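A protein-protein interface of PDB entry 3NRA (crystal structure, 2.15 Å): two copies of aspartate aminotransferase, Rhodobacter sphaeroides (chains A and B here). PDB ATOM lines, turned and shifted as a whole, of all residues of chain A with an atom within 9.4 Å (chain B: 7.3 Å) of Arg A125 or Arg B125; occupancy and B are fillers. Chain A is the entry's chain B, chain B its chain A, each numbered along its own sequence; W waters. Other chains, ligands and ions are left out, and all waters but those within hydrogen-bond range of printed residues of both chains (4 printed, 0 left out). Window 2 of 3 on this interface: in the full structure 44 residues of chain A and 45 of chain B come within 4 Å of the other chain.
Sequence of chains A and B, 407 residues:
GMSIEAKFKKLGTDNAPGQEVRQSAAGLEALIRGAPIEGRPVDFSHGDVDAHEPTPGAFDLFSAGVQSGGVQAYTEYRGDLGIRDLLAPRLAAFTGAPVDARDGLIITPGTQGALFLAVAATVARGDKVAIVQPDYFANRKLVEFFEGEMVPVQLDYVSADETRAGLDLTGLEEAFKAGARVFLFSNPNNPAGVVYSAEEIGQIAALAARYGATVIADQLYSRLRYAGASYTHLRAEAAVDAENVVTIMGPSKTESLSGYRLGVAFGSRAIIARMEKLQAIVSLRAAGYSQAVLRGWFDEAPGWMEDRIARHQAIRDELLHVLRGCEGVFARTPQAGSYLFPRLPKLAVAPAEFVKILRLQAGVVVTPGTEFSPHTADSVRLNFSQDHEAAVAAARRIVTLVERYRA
Water W1 lies within hydrogen-bond range of the backbone carbonyl oxygen (O) of Val A123, the backbone carbonyl oxygen (O) of Ala A120 and the side-chain amino group (NZ) of Lys B7. Water W4 bridges NZ of Lys A7 and O of Val B123. Water W3 lies within hydrogen-bond range of the backbone NH of Arg B125, the side-chain carboxylate of Glu A147 and the side-chain amino group of Lys A7. Water W2 lies within hydrogen-bond range of the backbone NH (N) of Arg A125 and the side-chain amino group (NZ) of Lys B7.
CD1 of Ile A4 touches C of Val B123, 3.6 Å away. CD1 of Ile A4 touches N of Ala B124 (3.5 Å). Ala A120 touches Ile B4. Ile B4 touches Thr A122 (CD1 to C, 3.5 Å). Val A123 touches Ile B4 (N to CD1, 3.6 Å). CD of Arg A125 touches NE of Arg B125 (3.3 Å).
Printed residues of chain B within 4 Å of Ala A120: Ile B4 (3.8 Å). Printed residues of chain B within 4 Å of Thr A122: Ile B4. Of the printed residues of chain B, Val A123 touches Ile B4. Ala A124 touches none of the printed residues of chain B. Val A143 touches none of the printed residues of chain B. Of the printed residues of chain A, Ile B4 touches Ala A120 (3.8 Å), Thr A122 (3.5 Å) and Val A123 (3.6 Å). Of the printed residues of chain A, Arg B125 touches Arg A125. The nearest residue of chain B that does not touch Arg A125 is Glu B147 (4.7 Å). The nearest residue of chain A that does not touch Arg B125 is Glu A147 (4.1 Å).
OE1 of Glu B147 is in salt-bridge range of NE of Arg B125, 3.3 Å away. The side-chain hydroxyl (OG1) of Thr A122 lies within hydrogen-bond range of the backbone carbonyl oxygen (O) of Val A119 (3.4 Å). The backbone NH (N) of Ala B124 sits at hydrogen-bond distance from the side-chain carboxylate (OD2) of Asp B127 (2.9 Å).
Ile A4 touches Val B123, and with the chains exchanged Val A123 touches Ile B4. Ile A4 touches Ala B124, but with the chains exchanged Ala A124 does not touch Ile B4 (4.1 Å). Arg B125 touches its own counterpart, Arg A125. Positions printed for both chains: 4, 7, 123, 124, 125, 126, 127, 128, 146, 147, 148 and 149. Of the 6 pairs that touch across the chains among the printed residues, 3 have their exchanged pair printed and touching as well.
Of the 12 printed residues of chain B, 4 touch a printed residue of chain A. Printed residues of chain B that touch a printed residue of chain A: Ile B4, Val B123, Ala B124 and Arg B125. Hydrophobic or aromatic side chains of chain B within 4 Å of the printed part of chain A: Ile B4 and Ala B124. Along chain B the printed residues that touch a printed residue of chain A span positions 4 to 125. Of the 21 printed residues of chain A, 5 touch a printed residue of chain B. Among the printed residues, 6 pairs touch across the chains. Among the printed residues, no Asp or Glu carboxylate lies within 4 Å of a Lys or Arg side-chain nitrogen of the other chain.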
ATOM      1  N   SER A   3      19.868  -5.971 -13.600  1.00  0.00           N
ATOM      2  CA  SER A   3      18.684  -6.782 -14.022  1.00  0.00           C
ATOM      3  C   SER A   3      17.798  -7.070 -12.822  1.00  0.00           C
ATOM      4  O   SER A   3      18.257  -7.633 -11.827  1.00  0.00           O
ATOM      5  CB  SER A   3      19.120  -8.103 -14.657  1.00  0.00           C
ATOM      6  OG  SER A   3      18.217  -9.160 -14.316  1.00  0.00           O
ATOM      7  N   ILE A   4      16.520  -6.725 -12.931  1.00  0.00           N
ATOM      8  CA  ILE A   4      15.591  -6.850 -11.792  1.00  0.00           C
ATOM      9  C   ILE A   4      15.490  -8.323 -11.284  1.00  0.00           C
ATOM     10  O   ILE A   4      15.455  -8.561 -10.067  1.00  0.00           O
ATOM     11  CB  ILE A   4      14.164  -6.292 -12.133  1.00  0.00           C
ATOM     12  CG1 ILE A   4      13.585  -5.548 -10.935  1.00  0.00           C
ATOM     13  CG2 ILE A   4      13.228  -7.403 -12.542  1.00  0.00           C
ATOM     14  CD1 ILE A   4      14.124  -4.117 -10.783  1.00  0.00           C
ATOM     15  N   LYS A   7      18.711  -9.471  -9.230  1.00  0.00           N
ATOM     16  CA  LYS A   7      18.690  -8.640  -8.008  1.00  0.00           C
ATOM     17  C   LYS A   7      17.819  -9.280  -6.951  1.00  0.00           C
ATOM     18  O   LYS A   7      18.263  -9.521  -5.846  1.00  0.00           O
ATOM     19  CB  LYS A   7      18.162  -7.240  -8.360  1.00  0.00           C
ATOM     20  CG  LYS A   7      18.223  -6.173  -7.238  1.00  0.00           C
ATOM     21  CD  LYS A   7      17.264  -4.987  -7.586  1.00  0.00           C
ATOM     22  CE  LYS A   7      17.845  -3.625  -7.216  1.00  0.00           C
ATOM     23  NZ  LYS A   7      16.928  -2.484  -7.598  1.00  0.00           N
ATOM     24  N   VAL A 119      20.560   1.515   6.176  1.00  0.00           N
ATOM     25  CA  VAL A 119      21.408   1.047   5.077  1.00  0.00           C
ATOM     26  C   VAL A 119      21.106   1.866   3.797  1.00  0.00           C
ATOM     27  O   VAL A 119      22.033   2.270   3.071  1.00  0.00           O
ATOM     28  CB  VAL A 119      21.220  -0.442   4.824  1.00  0.00           C
ATOM     29  CG1 VAL A 119      22.068  -0.900   3.620  1.00  0.00           C
ATOM     30  CG2 VAL A 119      21.568  -1.266   6.112  1.00  0.00           C
ATOM     31  N   ALA A 120      19.819   2.138   3.545  1.00  0.00           N
ATOM     32  CA  ALA A 120      19.414   2.939   2.355  1.00  0.00           C
ATOM     33  C   ALA A 120      20.031   4.327   2.375  1.00  0.00           C
ATOM     34  O   ALA A 120      20.440   4.839   1.335  1.00  0.00           O
ATOM     35  CB  ALA A 120      17.906   3.053   2.268  1.00  0.00           C
ATOM     36  N   THR A 122      22.882   5.182   3.769  1.00  0.00           N
ATOM     37  CA  THR A 122      24.323   5.150   3.917  1.00  0.00           C
ATOM     38  C   THR A 122      25.083   4.368   2.821  1.00  0.00           C
ATOM     39  O   THR A 122      26.269   4.586   2.648  1.00  0.00           O
ATOM     40  CB  THR A 122      24.732   4.614   5.310  1.00  0.00           C
ATOM     41  OG1 THR A 122      24.238   3.274   5.481  1.00  0.00           O
ATOM     42  CG2 THR A 122      24.182   5.505   6.415  1.00  0.00           C
ATOM     43  N   VAL A 123      24.401   3.493   2.070  1.00  0.00           N
ATOM     44  CA  VAL A 123      25.068   2.673   1.066  1.00  0.00           C
ATOM     45  C   VAL A 123      24.582   3.024  -0.364  1.00  0.00           C
ATOM     46  O   VAL A 123      23.405   2.935  -0.677  1.00  0.00           O
ATOM     47  CB  VAL A 123      24.875   1.178   1.329  1.00  0.00           C
ATOM     48  CG1 VAL A 123      25.622   0.357   0.269  1.00  0.00           C
ATOM     49  CG2 VAL A 123      25.342   0.801   2.774  1.00  0.00           C
ATOM     50  N   ALA A 124      25.500   3.484  -1.186  1.00  0.00           N
ATOM     51  CA  ALA A 124      25.231   3.709  -2.596  1.00  0.00           C
ATOM     52  C   ALA A 124      25.835   2.585  -3.405  1.00  0.00           C
ATOM     53  O   ALA A 124      26.676   1.831  -2.920  1.00  0.00           O
ATOM     54  CB  ALA A 124      25.824   5.052  -3.043  1.00  0.00           C
ATOM     55  N   ARG A 125      25.455   2.538  -4.667  1.00  0.00           N
ATOM     56  CA  ARG A 125      25.939   1.536  -5.593  1.00  0.00           C
ATOM     57  C   ARG A 125      27.490   1.490  -5.657  1.00  0.00           C
ATOM     58  O   ARG A 125      28.142   2.504  -5.926  1.00  0.00           O
ATOM     59  CB  ARG A 125      25.351   1.833  -6.965  1.00  0.00           C
ATOM     60  CG  ARG A 125      25.893   0.974  -8.090  1.00  0.00           C
ATOM     61  CD  ARG A 125      24.913   0.902  -9.248  1.00  0.00           C
ATOM     62  NE  ARG A 125      25.597   0.893 -10.539  1.00  0.00           N
ATOM     63  CZ  ARG A 125      26.021   1.984 -11.196  1.00  0.00           C
ATOM     64  NH1 ARG A 125      25.873   3.225 -10.682  1.00  0.00           N
ATOM     65  NH2 ARG A 125      26.613   1.838 -12.381  1.00  0.00           N
ATOM     66  N   GLY A 126      28.057   0.307  -5.386  1.00  0.00           N
ATOM     67  CA  GLY A 126      29.506   0.092  -5.440  1.00  0.00           C
ATOM     68  C   GLY A 126      30.265   0.394  -4.145  1.00  0.00           C
ATOM     69  O   GLY A 126      31.457   0.129  -4.056  1.00  0.00           O
ATOM     70  N   ASP A 127      29.591   0.947  -3.145  1.00  0.00           N
ATOM     71  CA  ASP A 127      30.250   1.224  -1.850  1.00  0.00           C
ATOM     72  C   ASP A 127      30.595  -0.061  -1.139  1.00  0.00           C
ATOM     73  O   ASP A 127      29.786  -0.961  -1.087  1.00  0.00           O
ATOM     74  CB  ASP A 127      29.350   2.037  -0.943  1.00  0.00           C
ATOM     75  CG  ASP A 127      29.213   3.463  -1.383  1.00  0.00           C
ATOM     76  OD1 ASP A 127      29.878   3.853  -2.364  1.00  0.00           O
ATOM     77  OD2 ASP A 127      28.427   4.207  -0.735  1.00  0.00           O
ATOM     78  N   LYS A 128      31.804  -0.131  -0.587  1.00  0.00           N
ATOM     79  CA  LYS A 128      32.182  -1.225   0.289  1.00  0.00           C
ATOM     80  C   LYS A 128      31.566  -1.085   1.705  1.00  0.00           C
ATOM     81  O   LYS A 128      31.586  -0.016   2.297  1.00  0.00           O
ATOM     82  CB  LYS A 128      33.686  -1.343   0.359  1.00  0.00           C
ATOM     83  CG  LYS A 128      34.258  -1.948  -0.907  1.00  0.00           C
ATOM     84  CD  LYS A 128      35.734  -1.735  -1.031  1.00  0.00           C
ATOM     85  CE  LYS A 128      36.249  -2.342  -2.323  1.00  0.00           C
ATOM     86  NZ  LYS A 128      37.454  -1.680  -2.787  1.00  0.00           N
ATOM     87  N   VAL A 129      30.986  -2.162   2.196  1.00  0.00           N
ATOM     88  CA  VAL A 129      30.364  -2.190   3.506  1.00  0.00           C
ATOM     89  C   VAL A 129      30.908  -3.357   4.289  1.00  0.00           C
ATOM     90  O   VAL A 129      30.863  -4.476   3.799  1.00  0.00           O
ATOM     91  CB  VAL A 129      28.824  -2.343   3.390  1.00  0.00           C
ATOM     92  CG1 VAL A 129      28.180  -2.237   4.775  1.00  0.00           C
ATOM     93  CG2 VAL A 129      28.246  -1.300   2.414  1.00  0.00           C
ATOM     94  N   LEU A 142      20.652  -6.611   2.599  1.00  0.00           N
ATOM     95  CA  LEU A 142      20.491  -5.181   2.472  1.00  0.00           C
ATOM     96  C   LEU A 142      21.622  -4.532   1.689  1.00  0.00           C
ATOM     97  O   LEU A 142      21.365  -3.750   0.748  1.00  0.00           O
ATOM     98  CB  LEU A 142      20.378  -4.543   3.836  1.00  0.00           C
ATOM     99  CG  LEU A 142      18.999  -4.684   4.462  1.00  0.00           C
ATOM    100  CD1 LEU A 142      19.069  -4.292   5.903  1.00  0.00           C
ATOM    101  CD2 LEU A 142      17.977  -3.825   3.704  1.00  0.00           C
ATOM    102  N   VAL A 143      22.863  -4.866   2.043  1.00  0.00           N
ATOM    103  CA  VAL A 143      24.032  -4.343   1.323  1.00  0.00           C
ATOM    104  C   VAL A 143      23.941  -4.676  -0.157  1.00  0.00           C
ATOM    105  O   VAL A 143      24.116  -3.816  -1.005  1.00  0.00           O
ATOM    106  CB  VAL A 143      25.380  -4.873   1.919  1.00  0.00           C
ATOM    107  CG1 VAL A 143      26.504  -4.511   1.036  1.00  0.00           C
ATOM    108  CG2 VAL A 143      25.606  -4.269   3.369  1.00  0.00           C
ATOM    109  N   GLU A 144      23.575  -5.899  -0.457  1.00  0.00           N
ATOM    110  CA  GLU A 144      23.577  -6.343  -1.825  1.00  0.00           C
ATOM    111  C   GLU A 144      22.359  -5.810  -2.637  1.00  0.00           C
ATOM    112  O   GLU A 144      22.508  -5.487  -3.818  1.00  0.00           O
ATOM    113  CB  GLU A 144      23.767  -7.881  -1.894  1.00  0.00           C
ATOM    114  CG  GLU A 144      25.314  -8.236  -1.687  1.00  0.00           C
ATOM    115  CD  GLU A 144      25.636  -9.722  -1.470  1.00  0.00           C
ATOM    116  OE1 GLU A 144      24.702 -10.546  -1.354  1.00  0.00           O
ATOM    117  OE2 GLU A 144      26.864 -10.047  -1.412  1.00  0.00           O
ATOM    118  N   PHE A 145      21.232  -5.577  -1.967  1.00  0.00           N
ATOM    119  CA  PHE A 145      20.086  -4.941  -2.595  1.00  0.00           C
ATOM    120  C   PHE A 145      20.375  -3.508  -3.037  1.00  0.00           C
ATOM    121  O   PHE A 145      19.924  -3.077  -4.096  1.00  0.00           O
ATOM    122  CB  PHE A 145      18.904  -4.911  -1.651  1.00  0.00           C
ATOM    123  CG  PHE A 145      17.657  -4.347  -2.278  1.00  0.00           C
ATOM    124  CD1 PHE A 145      17.035  -5.010  -3.315  1.00  0.00           C
ATOM    125  CD2 PHE A 145      17.129  -3.141  -1.856  1.00  0.00           C
ATOM    126  CE1 PHE A 145      15.869  -4.492  -3.889  1.00  0.00           C
ATOM    127  CE2 PHE A 145      15.975  -2.618  -2.457  1.00  0.00           C
ATOM    128  CZ  PHE A 145      15.364  -3.295  -3.465  1.00  0.00           C
ATOM    129  N   PHE A 146      21.143  -2.778  -2.235  1.00  0.00           N
ATOM    130  CA  PHE A 146      21.567  -1.458  -2.625  1.00  0.00           C
ATOM    131  C   PHE A 146      22.876  -1.467  -3.492  1.00  0.00           C
ATOM    132  O   PHE A 146      23.495  -0.426  -3.708  1.00  0.00           O
ATOM    133  CB  PHE A 146      21.649  -0.558  -1.390  1.00  0.00           C
ATOM    134  CG  PHE A 146      20.282  -0.195  -0.823  1.00  0.00           C
ATOM    135  CD1 PHE A 146      19.449   0.707  -1.496  1.00  0.00           C
ATOM    136  CD2 PHE A 146      19.813  -0.782   0.315  1.00  0.00           C
ATOM    137  CE1 PHE A 146      18.178   1.004  -1.007  1.00  0.00           C
ATOM    138  CE2 PHE A 146      18.544  -0.487   0.805  1.00  0.00           C
ATOM    139  CZ  PHE A 146      17.734   0.407   0.137  1.00  0.00           C
ATOM    140  N   GLU A 147      23.233  -2.642  -4.027  1.00  0.00           N
ATOM    141  CA  GLU A 147      24.385  -2.813  -4.927  1.00  0.00           C
ATOM    142  C   GLU A 147      25.717  -2.348  -4.321  1.00  0.00           C
ATOM    143  O   GLU A 147      26.661  -1.980  -5.055  1.00  0.00           O
ATOM    144  CB  GLU A 147      24.114  -2.150  -6.283  1.00  0.00           C
ATOM    145  CG  GLU A 147      22.806  -2.656  -6.983  1.00  0.00           C
ATOM    146  CD  GLU A 147      22.694  -2.195  -8.466  1.00  0.00           C
ATOM    147  OE1 GLU A 147      23.670  -2.403  -9.257  1.00  0.00           O
ATOM    148  OE2 GLU A 147      21.634  -1.620  -8.833  1.00  0.00           O
ATOM    149  N   GLY A 148      25.818  -2.447  -2.983  1.00  0.00           N
ATOM    150  CA  GLY A 148      27.094  -2.329  -2.292  1.00  0.00           C
ATOM    151  C   GLY A 148      27.859  -3.631  -2.363  1.00  0.00           C
ATOM    152  O   GLY A 148      27.291  -4.674  -2.697  1.00  0.00           O
ATOM    153  N   GLU A 149      29.142  -3.568  -2.029  1.00  0.00           N
ATOM    154  CA  GLU A 149      30.015  -4.736  -1.990  1.00  0.00           C
ATOM    155  C   GLU A 149      30.313  -5.071  -0.523  1.00  0.00           C
ATOM    156  O   GLU A 149      30.976  -4.290   0.177  1.00  0.00           O
ATOM    157  CB  GLU A 149      31.302  -4.417  -2.713  1.00  0.00           C
ATOM    158  CG  GLU A 149      32.283  -5.589  -2.844  1.00  0.00           C
ATOM    159  CD  GLU A 149      33.694  -5.145  -3.327  1.00  0.00           C
ATOM    160  OE1 GLU A 149      33.821  -4.056  -3.960  1.00  0.00           O
ATOM    161  OE2 GLU A 149      34.663  -5.873  -3.035  1.00  0.00           O
ATOM    162  N   ILE B   4      25.145   9.754  -2.962  1.00  0.00           N
ATOM    163  CA  ILE B   4      24.111   9.496  -1.942  1.00  0.00           C
ATOM    164  C   ILE B   4      23.450  10.806  -1.434  1.00  0.00           C
ATOM    165  O   ILE B   4      22.233  10.863  -1.271  1.00  0.00           O
ATOM    166  CB  ILE B   4      24.662   8.630  -0.763  1.00  0.00           C
ATOM    167  CG1 ILE B   4      23.531   8.164   0.143  1.00  0.00           C
ATOM    168  CG2 ILE B   4      25.719   9.377   0.042  1.00  0.00           C
ATOM    169  CD1 ILE B   4      23.690   6.724   0.569  1.00  0.00           C
ATOM    170  N   LYS B   7      21.151  11.924  -4.291  1.00  0.00           N
ATOM    171  CA  LYS B   7      20.007  11.008  -4.335  1.00  0.00           C
ATOM    172  C   LYS B   7      18.936  11.425  -3.331  1.00  0.00           C
ATOM    173  O   LYS B   7      17.761  11.559  -3.685  1.00  0.00           O
ATOM    174  CB  LYS B   7      20.477   9.566  -4.038  1.00  0.00           C
ATOM    175  CG  LYS B   7      19.420   8.432  -4.234  1.00  0.00           C
ATOM    176  CD  LYS B   7      19.973   7.114  -3.661  1.00  0.00           C
ATOM    177  CE  LYS B   7      19.455   5.885  -4.376  1.00  0.00           C
ATOM    178  NZ  LYS B   7      20.170   4.633  -3.958  1.00  0.00           N
ATOM    179  N   VAL B 123      11.173  -1.556 -11.220  1.00  0.00           N
ATOM    180  CA  VAL B 123      11.977  -0.488 -11.806  1.00  0.00           C
ATOM    181  C   VAL B 123      13.472  -0.657 -11.451  1.00  0.00           C
ATOM    182  O   VAL B 123      13.886  -0.426 -10.317  1.00  0.00           O
ATOM    183  CB  VAL B 123      11.496   0.877 -11.352  1.00  0.00           C
ATOM    184  CG1 VAL B 123      12.295   1.986 -12.059  1.00  0.00           C
ATOM    185  CG2 VAL B 123       9.983   1.024 -11.613  1.00  0.00           C
ATOM    186  N   ALA B 124      14.255  -1.079 -12.441  1.00  0.00           N
ATOM    187  CA  ALA B 124      15.704  -1.146 -12.330  1.00  0.00           C
ATOM    188  C   ALA B 124      16.318   0.177 -12.771  1.00  0.00           C
ATOM    189  O   ALA B 124      15.671   0.982 -13.437  1.00  0.00           O
ATOM    190  CB  ALA B 124      16.237  -2.290 -13.207  1.00  0.00           C
ATOM    191  N   ARG B 125      17.589   0.362 -12.441  1.00  0.00           N
ATOM    192  CA  ARG B 125      18.328   1.567 -12.805  1.00  0.00           C
ATOM    193  C   ARG B 125      18.259   1.813 -14.319  1.00  0.00           C
ATOM    194  O   ARG B 125      18.543   0.919 -15.095  1.00  0.00           O
ATOM    195  CB  ARG B 125      19.791   1.404 -12.370  1.00  0.00           C
ATOM    196  CG  ARG B 125      20.731   2.605 -12.688  1.00  0.00           C
ATOM    197  CD  ARG B 125      22.177   2.345 -12.149  1.00  0.00           C
ATOM    198  NE  ARG B 125      22.178   2.029 -10.708  1.00  0.00           N
ATOM    199  N   GLY B 126      17.866   3.033 -14.717  1.00  0.00           N
ATOM    200  CA  GLY B 126      17.814   3.429 -16.141  1.00  0.00           C
ATOM    201  C   GLY B 126      16.467   3.175 -16.847  1.00  0.00           C
ATOM    202  O   GLY B 126      16.213   3.728 -17.937  1.00  0.00           O
ATOM    203  N   ASP B 127      15.603   2.359 -16.242  1.00  0.00           N
ATOM    204  CA  ASP B 127      14.320   2.038 -16.851  1.00  0.00           C
ATOM    205  C   ASP B 127      13.436   3.296 -16.967  1.00  0.00           C
ATOM    206  O   ASP B 127      13.285   4.065 -15.990  1.00  0.00           O
ATOM    207  CB  ASP B 127      13.564   1.002 -16.014  1.00  0.00           C
ATOM    208  CG  ASP B 127      14.186  -0.378 -16.060  1.00  0.00           C
ATOM    209  OD1 ASP B 127      15.052  -0.636 -16.908  1.00  0.00           O
ATOM    210  OD2 ASP B 127      13.751  -1.232 -15.253  1.00  0.00           O
ATOM    211  N   LYS B 128      12.785   3.435 -18.124  1.00  0.00           N
ATOM    212  CA  LYS B 128      11.757   4.433 -18.330  1.00  0.00           C
ATOM    213  C   LYS B 128      10.427   4.016 -17.671  1.00  0.00           C
ATOM    214  O   LYS B 128       9.984   2.889 -17.813  1.00  0.00           O
ATOM    215  CB  LYS B 128      11.554   4.698 -19.838  1.00  0.00           C
ATOM    216  CG  LYS B 128      12.667   5.560 -20.460  1.00  0.00           C
ATOM    217  CD  LYS B 128      12.650   5.503 -21.999  1.00  0.00           C
ATOM    218  CE  LYS B 128      13.705   6.475 -22.659  1.00  0.00           C
ATOM    219  NZ  LYS B 128      15.113   6.214 -22.208  1.00  0.00           N
ATOM    220  N   PHE B 146      14.779   4.834  -7.239  1.00  0.00           N
ATOM    221  CA  PHE B 146      15.327   3.629  -7.912  1.00  0.00           C
ATOM    222  C   PHE B 146      16.088   3.921  -9.206  1.00  0.00           C
ATOM    223  O   PHE B 146      16.434   3.007  -9.933  1.00  0.00           O
ATOM    224  CB  PHE B 146      14.205   2.606  -8.124  1.00  0.00           C
ATOM    225  CG  PHE B 146      13.700   2.046  -6.854  1.00  0.00           C
ATOM    226  CD1 PHE B 146      14.471   1.144  -6.140  1.00  0.00           C
ATOM    227  CD2 PHE B 146      12.525   2.509  -6.286  1.00  0.00           C
ATOM    228  CE1 PHE B 146      14.038   0.661  -4.905  1.00  0.00           C
ATOM    229  CE2 PHE B 146      12.098   2.039  -5.060  1.00  0.00           C
ATOM    230  CZ  PHE B 146      12.849   1.111  -4.373  1.00  0.00           C
ATOM    231  N   GLU B 147      16.375   5.204  -9.454  1.00  0.00           N
ATOM    232  CA  GLU B 147      17.141   5.669 -10.625  1.00  0.00           C
ATOM    233  C   GLU B 147      16.491   5.306 -11.963  1.00  0.00           C
ATOM    234  O   GLU B 147      17.176   5.101 -12.973  1.00  0.00           O
ATOM    235  CB  GLU B 147      18.609   5.194 -10.549  1.00  0.00           C
ATOM    236  CG  GLU B 147      19.355   5.706  -9.303  1.00  0.00           C
ATOM    237  CD  GLU B 147      20.575   4.865  -8.972  1.00  0.00           C
ATOM    238  OE1 GLU B 147      21.650   5.070  -9.610  1.00  0.00           O
ATOM    239  OE2 GLU B 147      20.455   3.974  -8.093  1.00  0.00           O
ATOM    240  N   GLY B 148      15.160   5.259 -11.964  1.00  0.00           N
ATOM    241  CA  GLY B 148      14.402   5.205 -13.182  1.00  0.00           C
ATOM    242  C   GLY B 148      14.370   6.580 -13.838  1.00  0.00           C
ATOM    243  O   GLY B 148      14.766   7.599 -13.221  1.00  0.00           O
ATOM    244  N   GLU B 149      13.944   6.597 -15.089  1.00  0.00           N
ATOM    245  CA  GLU B 149      13.691   7.845 -15.840  1.00  0.00           C
ATOM    246  C   GLU B 149      12.185   8.031 -15.967  1.00  0.00           C
ATOM    247  O   GLU B 149      11.518   7.260 -16.632  1.00  0.00           O
ATOM    248  CB  GLU B 149      14.330   7.751 -17.227  1.00  0.00           C
ATOM    249  CG  GLU B 149      14.222   9.048 -18.106  1.00  0.00           C
ATOM    250  CD  GLU B 149      14.673   8.810 -19.559  1.00  0.00           C
ATOM    251  OE1 GLU B 149      15.321   7.767 -19.820  1.00  0.00           O
ATOM    252  OE2 GLU B 149      14.348   9.653 -20.431  1.00  0.00           O
HETATM  253  O   HOH W   1      21.276   4.174  -1.185  1.00  0.00           O
HETATM  254  O   HOH W   2      23.148   4.534  -5.622  1.00  0.00           O
HETATM  255  O   HOH W   3      18.808  -1.545 -10.396  1.00  0.00           O
HETATM  256  O   HOH W   4      14.433  -2.105  -8.176  1.00  0.00           O
